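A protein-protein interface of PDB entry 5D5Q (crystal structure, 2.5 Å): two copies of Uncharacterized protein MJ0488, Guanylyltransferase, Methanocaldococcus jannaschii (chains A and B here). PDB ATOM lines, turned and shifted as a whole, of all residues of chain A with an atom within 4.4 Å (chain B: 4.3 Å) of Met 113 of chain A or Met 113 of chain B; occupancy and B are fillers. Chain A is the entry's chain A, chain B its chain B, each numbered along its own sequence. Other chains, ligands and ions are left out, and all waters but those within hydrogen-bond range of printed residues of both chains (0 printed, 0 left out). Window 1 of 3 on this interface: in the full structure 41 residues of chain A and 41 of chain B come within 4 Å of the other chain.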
ATOM      1  N   ALA A  83     -27.020 -27.485 -16.175  1.00  0.00           N
ATOM      2  CA  ALA A  83     -28.192 -27.123 -16.974  1.00  0.00           C
ATOM      3  C   ALA A  83     -28.590 -28.256 -17.917  1.00  0.00           C
ATOM      4  O   ALA A  83     -29.754 -28.680 -17.962  1.00  0.00           O
ATOM      5  CB  ALA A  83     -27.925 -25.851 -17.759  1.00  0.00           C
ATOM      6  N   ALA A 101     -34.330 -25.822 -20.056  1.00  0.00           N
ATOM      7  CA  ALA A 101     -33.603 -25.930 -18.797  1.00  0.00           C
ATOM      8  C   ALA A 101     -32.726 -24.714 -18.540  1.00  0.00           C
ATOM      9  O   ALA A 101     -32.263 -24.064 -19.472  1.00  0.00           O
ATOM     10  CB  ALA A 101     -32.762 -27.197 -18.784  1.00  0.00           C
ATOM     11  N   ARG A 102     -32.515 -24.404 -17.266  1.00  0.00           N
ATOM     12  CA  ARG A 102     -31.639 -23.306 -16.879  1.00  0.00           C
ATOM     13  C   ARG A 102     -30.839 -23.693 -15.647  1.00  0.00           C
ATOM     14  O   ARG A 102     -31.401 -24.149 -14.651  1.00  0.00           O
ATOM     15  CB  ARG A 102     -32.430 -22.028 -16.600  1.00  0.00           C
ATOM     16  CG  ARG A 102     -31.560 -20.777 -16.587  1.00  0.00           C
ATOM     17  CD  ARG A 102     -32.201 -19.644 -15.805  1.00  0.00           C
ATOM     18  NE  ARG A 102     -31.269 -18.537 -15.594  1.00  0.00           N
ATOM     19  CZ  ARG A 102     -30.497 -18.401 -14.521  1.00  0.00           C
ATOM     20  NH1 ARG A 102     -29.678 -17.364 -14.416  1.00  0.00           N
ATOM     21  NH2 ARG A 102     -30.543 -19.303 -13.549  1.00  0.00           N
ATOM     22  N   GLY A 103     -29.525 -23.515 -15.716  1.00  0.00           N
ATOM     23  CA  GLY A 103     -28.677 -23.858 -14.590  1.00  0.00           C
ATOM     24  C   GLY A 103     -27.279 -23.308 -14.745  1.00  0.00           C
ATOM     25  O   GLY A 103     -27.040 -22.429 -15.568  1.00  0.00           O
ATOM     26  N   LEU A 105     -23.499 -23.275 -16.004  1.00  0.00           N
ATOM     27  CA  LEU A 105     -22.857 -23.748 -17.225  1.00  0.00           C
ATOM     28  C   LEU A 105     -21.988 -24.976 -16.970  1.00  0.00           C
ATOM     29  O   LEU A 105     -22.245 -26.052 -17.508  1.00  0.00           O
ATOM     30  CB  LEU A 105     -22.014 -22.633 -17.848  1.00  0.00           C
ATOM     31  CG  LEU A 105     -21.121 -23.046 -19.020  1.00  0.00           C
ATOM     32  CD1 LEU A 105     -21.962 -23.519 -20.194  1.00  0.00           C
ATOM     33  CD2 LEU A 105     -20.211 -21.901 -19.433  1.00  0.00           C
ATOM     34  N   SER A 112     -24.240 -18.589 -16.035  1.00  0.00           N
ATOM     35  CA  SER A 112     -25.435 -19.398 -16.244  1.00  0.00           C
ATOM     36  C   SER A 112     -25.673 -19.760 -17.705  1.00  0.00           C
ATOM     37  O   SER A 112     -25.225 -19.063 -18.620  1.00  0.00           O
ATOM     38  CB  SER A 112     -26.665 -18.672 -15.693  1.00  0.00           C
ATOM     39  OG  SER A 112     -27.031 -17.583 -16.522  1.00  0.00           O
ATOM     40  N   MET A 113     -26.407 -20.852 -17.901  1.00  0.00           N
ATOM     41  CA  MET A 113     -26.806 -21.315 -19.223  1.00  0.00           C
ATOM     42  C   MET A 113     -28.273 -21.728 -19.250  1.00  0.00           C
ATOM     43  O   MET A 113     -28.756 -22.430 -18.352  1.00  0.00           O
ATOM     44  CB  MET A 113     -25.937 -22.494 -19.674  1.00  0.00           C
ATOM     45  CG  MET A 113     -26.489 -23.225 -20.897  1.00  0.00           C
ATOM     46  SD  MET A 113     -25.522 -24.650 -21.431  1.00  0.00           S
ATOM     47  CE  MET A 113     -24.575 -23.931 -22.768  1.00  0.00           C
ATOM     48  N   LEU A 114     -28.976 -21.274 -20.284  1.00  0.00           N
ATOM     49  CA  LEU A 114     -30.297 -21.791 -20.610  1.00  0.00           C
ATOM     50  C   LEU A 114     -30.180 -22.589 -21.900  1.00  0.00           C
ATOM     51  O   LEU A 114     -29.564 -22.132 -22.860  1.00  0.00           O
ATOM     52  CB  LEU A 114     -31.315 -20.656 -20.754  1.00  0.00           C
ATOM     53  CG  LEU A 114     -32.767 -21.003 -21.109  1.00  0.00           C
ATOM     54  CD1 LEU A 114     -33.711 -19.994 -20.475  1.00  0.00           C
ATOM     55  CD2 LEU A 114     -32.992 -21.049 -22.616  1.00  0.00           C
ATOM     56  N   VAL A 115     -30.768 -23.778 -21.921  1.00  0.00           N
ATOM     57  CA  VAL A 115     -30.659 -24.657 -23.076  1.00  0.00           C
ATOM     58  C   VAL A 115     -32.025 -25.231 -23.458  1.00  0.00           C
ATOM     59  O   VAL A 115     -32.875 -25.480 -22.595  1.00  0.00           O
ATOM     60  CB  VAL A 115     -29.650 -25.805 -22.808  1.00  0.00           C
ATOM     61  CG1 VAL A 115     -30.136 -26.701 -21.675  1.00  0.00           C
ATOM     62  CG2 VAL A 115     -29.390 -26.615 -24.072  1.00  0.00           C
ATOM     63  N   ALA A 126     -29.187 -22.342 -27.256  1.00  0.00           N
ATOM     64  CA  ALA A 126     -28.786 -22.045 -25.889  1.00  0.00           C
ATOM     65  C   ALA A 126     -28.344 -20.596 -25.754  1.00  0.00           C
ATOM     66  O   ALA A 126     -28.067 -19.928 -26.746  1.00  0.00           O
ATOM     67  CB  ALA A 126     -27.673 -22.980 -25.448  1.00  0.00           C
ATOM     68  N   SER A 127     -28.278 -20.112 -24.519  1.00  0.00           N
ATOM     69  CA  SER A 127     -27.764 -18.774 -24.262  1.00  0.00           C
ATOM     70  C   SER A 127     -27.137 -18.675 -22.879  1.00  0.00           C
ATOM     71  O   SER A 127     -27.490 -19.423 -21.967  1.00  0.00           O
ATOM     72  CB  SER A 127     -28.876 -17.745 -24.413  1.00  0.00           C
ATOM     73  OG  SER A 127     -29.938 -18.042 -23.530  1.00  0.00           O
ATOM     74  N   LEU A 128     -26.208 -17.737 -22.729  1.00  0.00           N
ATOM     75  CA  LEU A 128     -25.416 -17.642 -21.513  1.00  0.00           C
ATOM     76  C   LEU A 128     -25.550 -16.286 -20.839  1.00  0.00           C
ATOM     77  O   LEU A 128     -25.796 -15.275 -21.497  1.00  0.00           O
ATOM     78  CB  LEU A 128     -23.943 -17.909 -21.829  1.00  0.00           C
ATOM     79  CG  LEU A 128     -23.665 -19.179 -22.633  1.00  0.00           C
ATOM     80  CD1 LEU A 128     -22.211 -19.244 -23.043  1.00  0.00           C
ATOM     81  CD2 LEU A 128     -24.047 -20.406 -21.837  1.00  0.00           C
ATOM     82  N   ALA B  83     -18.230 -28.983 -30.215  1.00  0.00           N
ATOM     83  CA  ALA B  83     -17.211 -28.128 -29.603  1.00  0.00           C
ATOM     84  C   ALA B  83     -16.604 -28.768 -28.356  1.00  0.00           C
ATOM     85  O   ALA B  83     -15.375 -28.862 -28.217  1.00  0.00           O
ATOM     86  CB  ALA B  83     -17.804 -26.769 -29.264  1.00  0.00           C
ATOM     87  N   ALA B 101     -11.562 -24.571 -27.342  1.00  0.00           N
ATOM     88  CA  ALA B 101     -12.190 -25.337 -28.406  1.00  0.00           C
ATOM     89  C   ALA B 101     -13.293 -24.514 -29.026  1.00  0.00           C
ATOM     90  O   ALA B 101     -13.914 -23.692 -28.359  1.00  0.00           O
ATOM     91  CB  ALA B 101     -12.736 -26.649 -27.875  1.00  0.00           C
ATOM     92  N   ARG B 102     -13.530 -24.719 -30.312  1.00  0.00           N
ATOM     93  CA  ARG B 102     -14.583 -23.978 -30.968  1.00  0.00           C
ATOM     94  C   ARG B 102     -15.268 -24.879 -31.986  1.00  0.00           C
ATOM     95  O   ARG B 102     -14.599 -25.518 -32.795  1.00  0.00           O
ATOM     96  CB  ARG B 102     -14.014 -22.732 -31.643  1.00  0.00           C
ATOM     97  CG  ARG B 102     -15.047 -21.663 -31.880  1.00  0.00           C
ATOM     98  CD  ARG B 102     -15.697 -21.823 -33.220  1.00  0.00           C
ATOM     99  NE  ARG B 102     -16.555 -20.694 -33.543  1.00  0.00           N
ATOM    100  CZ  ARG B 102     -17.350 -20.666 -34.602  1.00  0.00           C
ATOM    101  NH1 ARG B 102     -18.105 -19.605 -34.854  1.00  0.00           N
ATOM    102  NH2 ARG B 102     -17.411 -21.723 -35.394  1.00  0.00           N
ATOM    103  N   GLY B 103     -16.593 -24.938 -31.955  1.00  0.00           N
ATOM    104  CA  GLY B 103     -17.302 -25.791 -32.894  1.00  0.00           C
ATOM    105  C   GLY B 103     -18.786 -25.513 -32.949  1.00  0.00           C
ATOM    106  O   GLY B 103     -19.238 -24.463 -32.509  1.00  0.00           O
ATOM    107  N   LEU B 105     -22.532 -25.751 -31.727  1.00  0.00           N
ATOM    108  CA  LEU B 105     -23.109 -25.865 -30.391  1.00  0.00           C
ATOM    109  C   LEU B 105     -23.691 -27.255 -30.160  1.00  0.00           C
ATOM    110  O   LEU B 105     -23.254 -27.976 -29.263  1.00  0.00           O
ATOM    111  CB  LEU B 105     -24.188 -24.803 -30.174  1.00  0.00           C
ATOM    112  CG  LEU B 105     -24.995 -24.957 -28.883  1.00  0.00           C
ATOM    113  CD1 LEU B 105     -24.092 -24.788 -27.669  1.00  0.00           C
ATOM    114  CD2 LEU B 105     -26.145 -23.964 -28.845  1.00  0.00           C
ATOM    115  N   SER B 112     -22.928 -21.659 -33.213  1.00  0.00           N
ATOM    116  CA  SER B 112     -21.609 -22.086 -32.749  1.00  0.00           C
ATOM    117  C   SER B 112     -21.368 -21.832 -31.264  1.00  0.00           C
ATOM    118  O   SER B 112     -22.047 -21.024 -30.636  1.00  0.00           O
ATOM    119  CB  SER B 112     -20.511 -21.406 -33.565  1.00  0.00           C
ATOM    120  OG  SER B 112     -20.376 -20.044 -33.215  1.00  0.00           O
ATOM    121  N   MET B 113     -20.405 -22.565 -30.714  1.00  0.00           N
ATOM    122  CA  MET B 113     -19.965 -22.403 -29.334  1.00  0.00           C
ATOM    123  C   MET B 113     -18.440 -22.434 -29.227  1.00  0.00           C
ATOM    124  O   MET B 113     -17.779 -23.280 -29.843  1.00  0.00           O
ATOM    125  CB  MET B 113     -20.569 -23.491 -28.446  1.00  0.00           C
ATOM    126  CG  MET B 113     -19.918 -23.582 -27.076  1.00  0.00           C
ATOM    127  SD  MET B 113     -20.572 -24.898 -26.029  1.00  0.00           S
ATOM    128  CE  MET B 113     -21.693 -23.980 -24.981  1.00  0.00           C
ATOM    129  N   LEU B 114     -17.889 -21.500 -28.455  1.00  0.00           N
ATOM    130  CA  LEU B 114     -16.487 -21.557 -28.047  1.00  0.00           C
ATOM    131  C   LEU B 114     -16.420 -21.867 -26.554  1.00  0.00           C
ATOM    132  O   LEU B 114     -17.160 -21.284 -25.767  1.00  0.00           O
ATOM    133  CB  LEU B 114     -15.764 -20.244 -28.368  1.00  0.00           C
ATOM    134  CG  LEU B 114     -14.280 -20.104 -28.002  1.00  0.00           C
ATOM    135  CD1 LEU B 114     -13.580 -19.199 -29.002  1.00  0.00           C
ATOM    136  CD2 LEU B 114     -14.083 -19.560 -26.590  1.00  0.00           C
ATOM    137  N   VAL B 115     -15.534 -22.785 -26.173  1.00  0.00           N
ATOM    138  CA  VAL B 115     -15.421 -23.230 -24.784  1.00  0.00           C
ATOM    139  C   VAL B 115     -13.980 -23.229 -24.287  1.00  0.00           C
ATOM    140  O   VAL B 115     -13.046 -23.504 -25.049  1.00  0.00           O
ATOM    141  CB  VAL B 115     -15.965 -24.665 -24.589  1.00  0.00           C
ATOM    142  CG1 VAL B 115     -16.461 -24.856 -23.162  1.00  0.00           C
ATOM    143  CG2 VAL B 115     -17.062 -24.977 -25.582  1.00  0.00           C
ATOM    144  N   ALA B 126     -17.637 -20.039 -21.602  1.00  0.00           N
ATOM    145  CA  ALA B 126     -18.057 -20.328 -22.964  1.00  0.00           C
ATOM    146  C   ALA B 126     -18.796 -19.146 -23.570  1.00  0.00           C
ATOM    147  O   ALA B 126     -19.202 -18.228 -22.863  1.00  0.00           O
ATOM    148  CB  ALA B 126     -18.933 -21.569 -22.998  1.00  0.00           C
ATOM    149  N   SER B 127     -18.961 -19.167 -24.886  1.00  0.00           N
ATOM    150  CA  SER B 127     -19.757 -18.150 -25.558  1.00  0.00           C
ATOM    151  C   SER B 127     -20.399 -18.710 -26.819  1.00  0.00           C
ATOM    152  O   SER B 127     -19.888 -19.656 -27.421  1.00  0.00           O
ATOM    153  CB  SER B 127     -18.895 -16.935 -25.887  1.00  0.00           C
ATOM    154  OG  SER B 127     -17.799 -17.315 -26.694  1.00  0.00           O
ATOM    155  N   LEU B 128     -21.519 -18.116 -27.216  1.00  0.00           N
ATOM    156  CA  LEU B 128     -22.318 -18.657 -28.306  1.00  0.00           C
ATOM    157  C   LEU B 128     -22.487 -17.667 -29.443  1.00  0.00           C
ATOM    158  O   LEU B 128     -22.474 -16.453 -29.241  1.00  0.00           O
ATOM    159  CB  LEU B 128     -23.688 -19.094 -27.789  1.00  0.00           C
ATOM    160  CG  LEU B 128     -23.607 -20.016 -26.576  1.00  0.00           C
ATOM    161  CD1 LEU B 128     -24.974 -20.271 -25.993  1.00  0.00           C
ATOM    162  CD2 LEU B 128     -22.955 -21.317 -26.982  1.00  0.00           C
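Of the 12 printed residues of chain A, 5 touch a printed residue of chain B. Of the 12 printed residues of chain B, 5 touch a printed residue of chain A. Printed residues of chain B that touch a printed residue of chain A: Leu 105, Met 113, Ala 126, Ser 127 and Leu 128. Hydrophobic or aromatic side chains of chain B that line the printed part of chain A: Leu 105, Met 113, Ala 126 and Leu 128. Among the printed residues, no Asp or Glu carboxylate lies within 4 Å of a Lys or Arg side-chain nitrogen of the other chain.
CD2 of Leu 105 of chain A touches CB of Ala 126 of chain B (3.8 Å). Met 113 of chain B touches Met 113 of chain A (CE to CE, 3.6 Å). N of Ala 126 of chain A touches CD2 of Leu 105 of chain B, at 3.8 Å. Leu 128 of chain B touches Ala 126 of chain A (CD1 to O, 3.2 Å). Ser 127 of chain A touches Leu 128 of chain B (CA to CD1, 3.6 Å). Ala 126 of chain B touches Leu 128 of chain A. CD1 of Leu 128 of chain A touches CA of Ser 127 of chain B (3.7 Å). Leu 128 of chain B touches Leu 128 of chain A.
Leu 105 of chain A touches Ala 126 of chain B, and with the chains exchanged Ala 126 of chain A touches Leu 105 of chain B. Ala 126 of chain A touches Leu 128 of chain B, and with the chains exchanged Leu 128 of chain A touches Ala 126 of chain B. Ser 127 of chain A touches Leu 128 of chain B, and with the chains exchanged Leu 128 of chain A touches Ser 127 of chain B. Leu 128 of chain B touches its own counterpart, Leu 128 of chain A. 12 positions are printed for both chains. Of the 8 pairs that touch across the chains among the printed residues, 8 have their exchanged pair printed and touching as well.
Ala 101 of chain A touches none of the printed residues of chain B. Printed residues of chain B within 4 Å of Leu 105 of chain A: Ala 126. Of the printed residues of chain B, Met 113 of chain A touches Met 113. Of the printed residues of chain B, Leu 128 of chain A touches Ala 126, Ser 127 and Leu 128. Of the printed residues of chain A, Leu 105 of chain B touches Ala 126. Leu 114 of chain B touches none of the printed residues of chain A. Of the printed residues of chain A, Ser 127 of chain B touches Leu 128.
The backbone NH of Met 113 of chain A sits at hydrogen-bond distance from the backbone carbonyl oxygen of Gly 103 of chain A. N of Leu 114 of chain A sits at hydrogen-bond distance from O of Ser 127 of chain A (2.9 Å). The backbone carbonyl oxygen (O) of Gly 103 of chain B sits at hydrogen-bond distance from the backbone NH (N) of Met 113 of chain B (2.9 Å). The backbone carbonyl oxygen (O) of Ser 127 of chain B is in hydrogen-bond range of the backbone NH (N) of Leu 114 of chain B.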
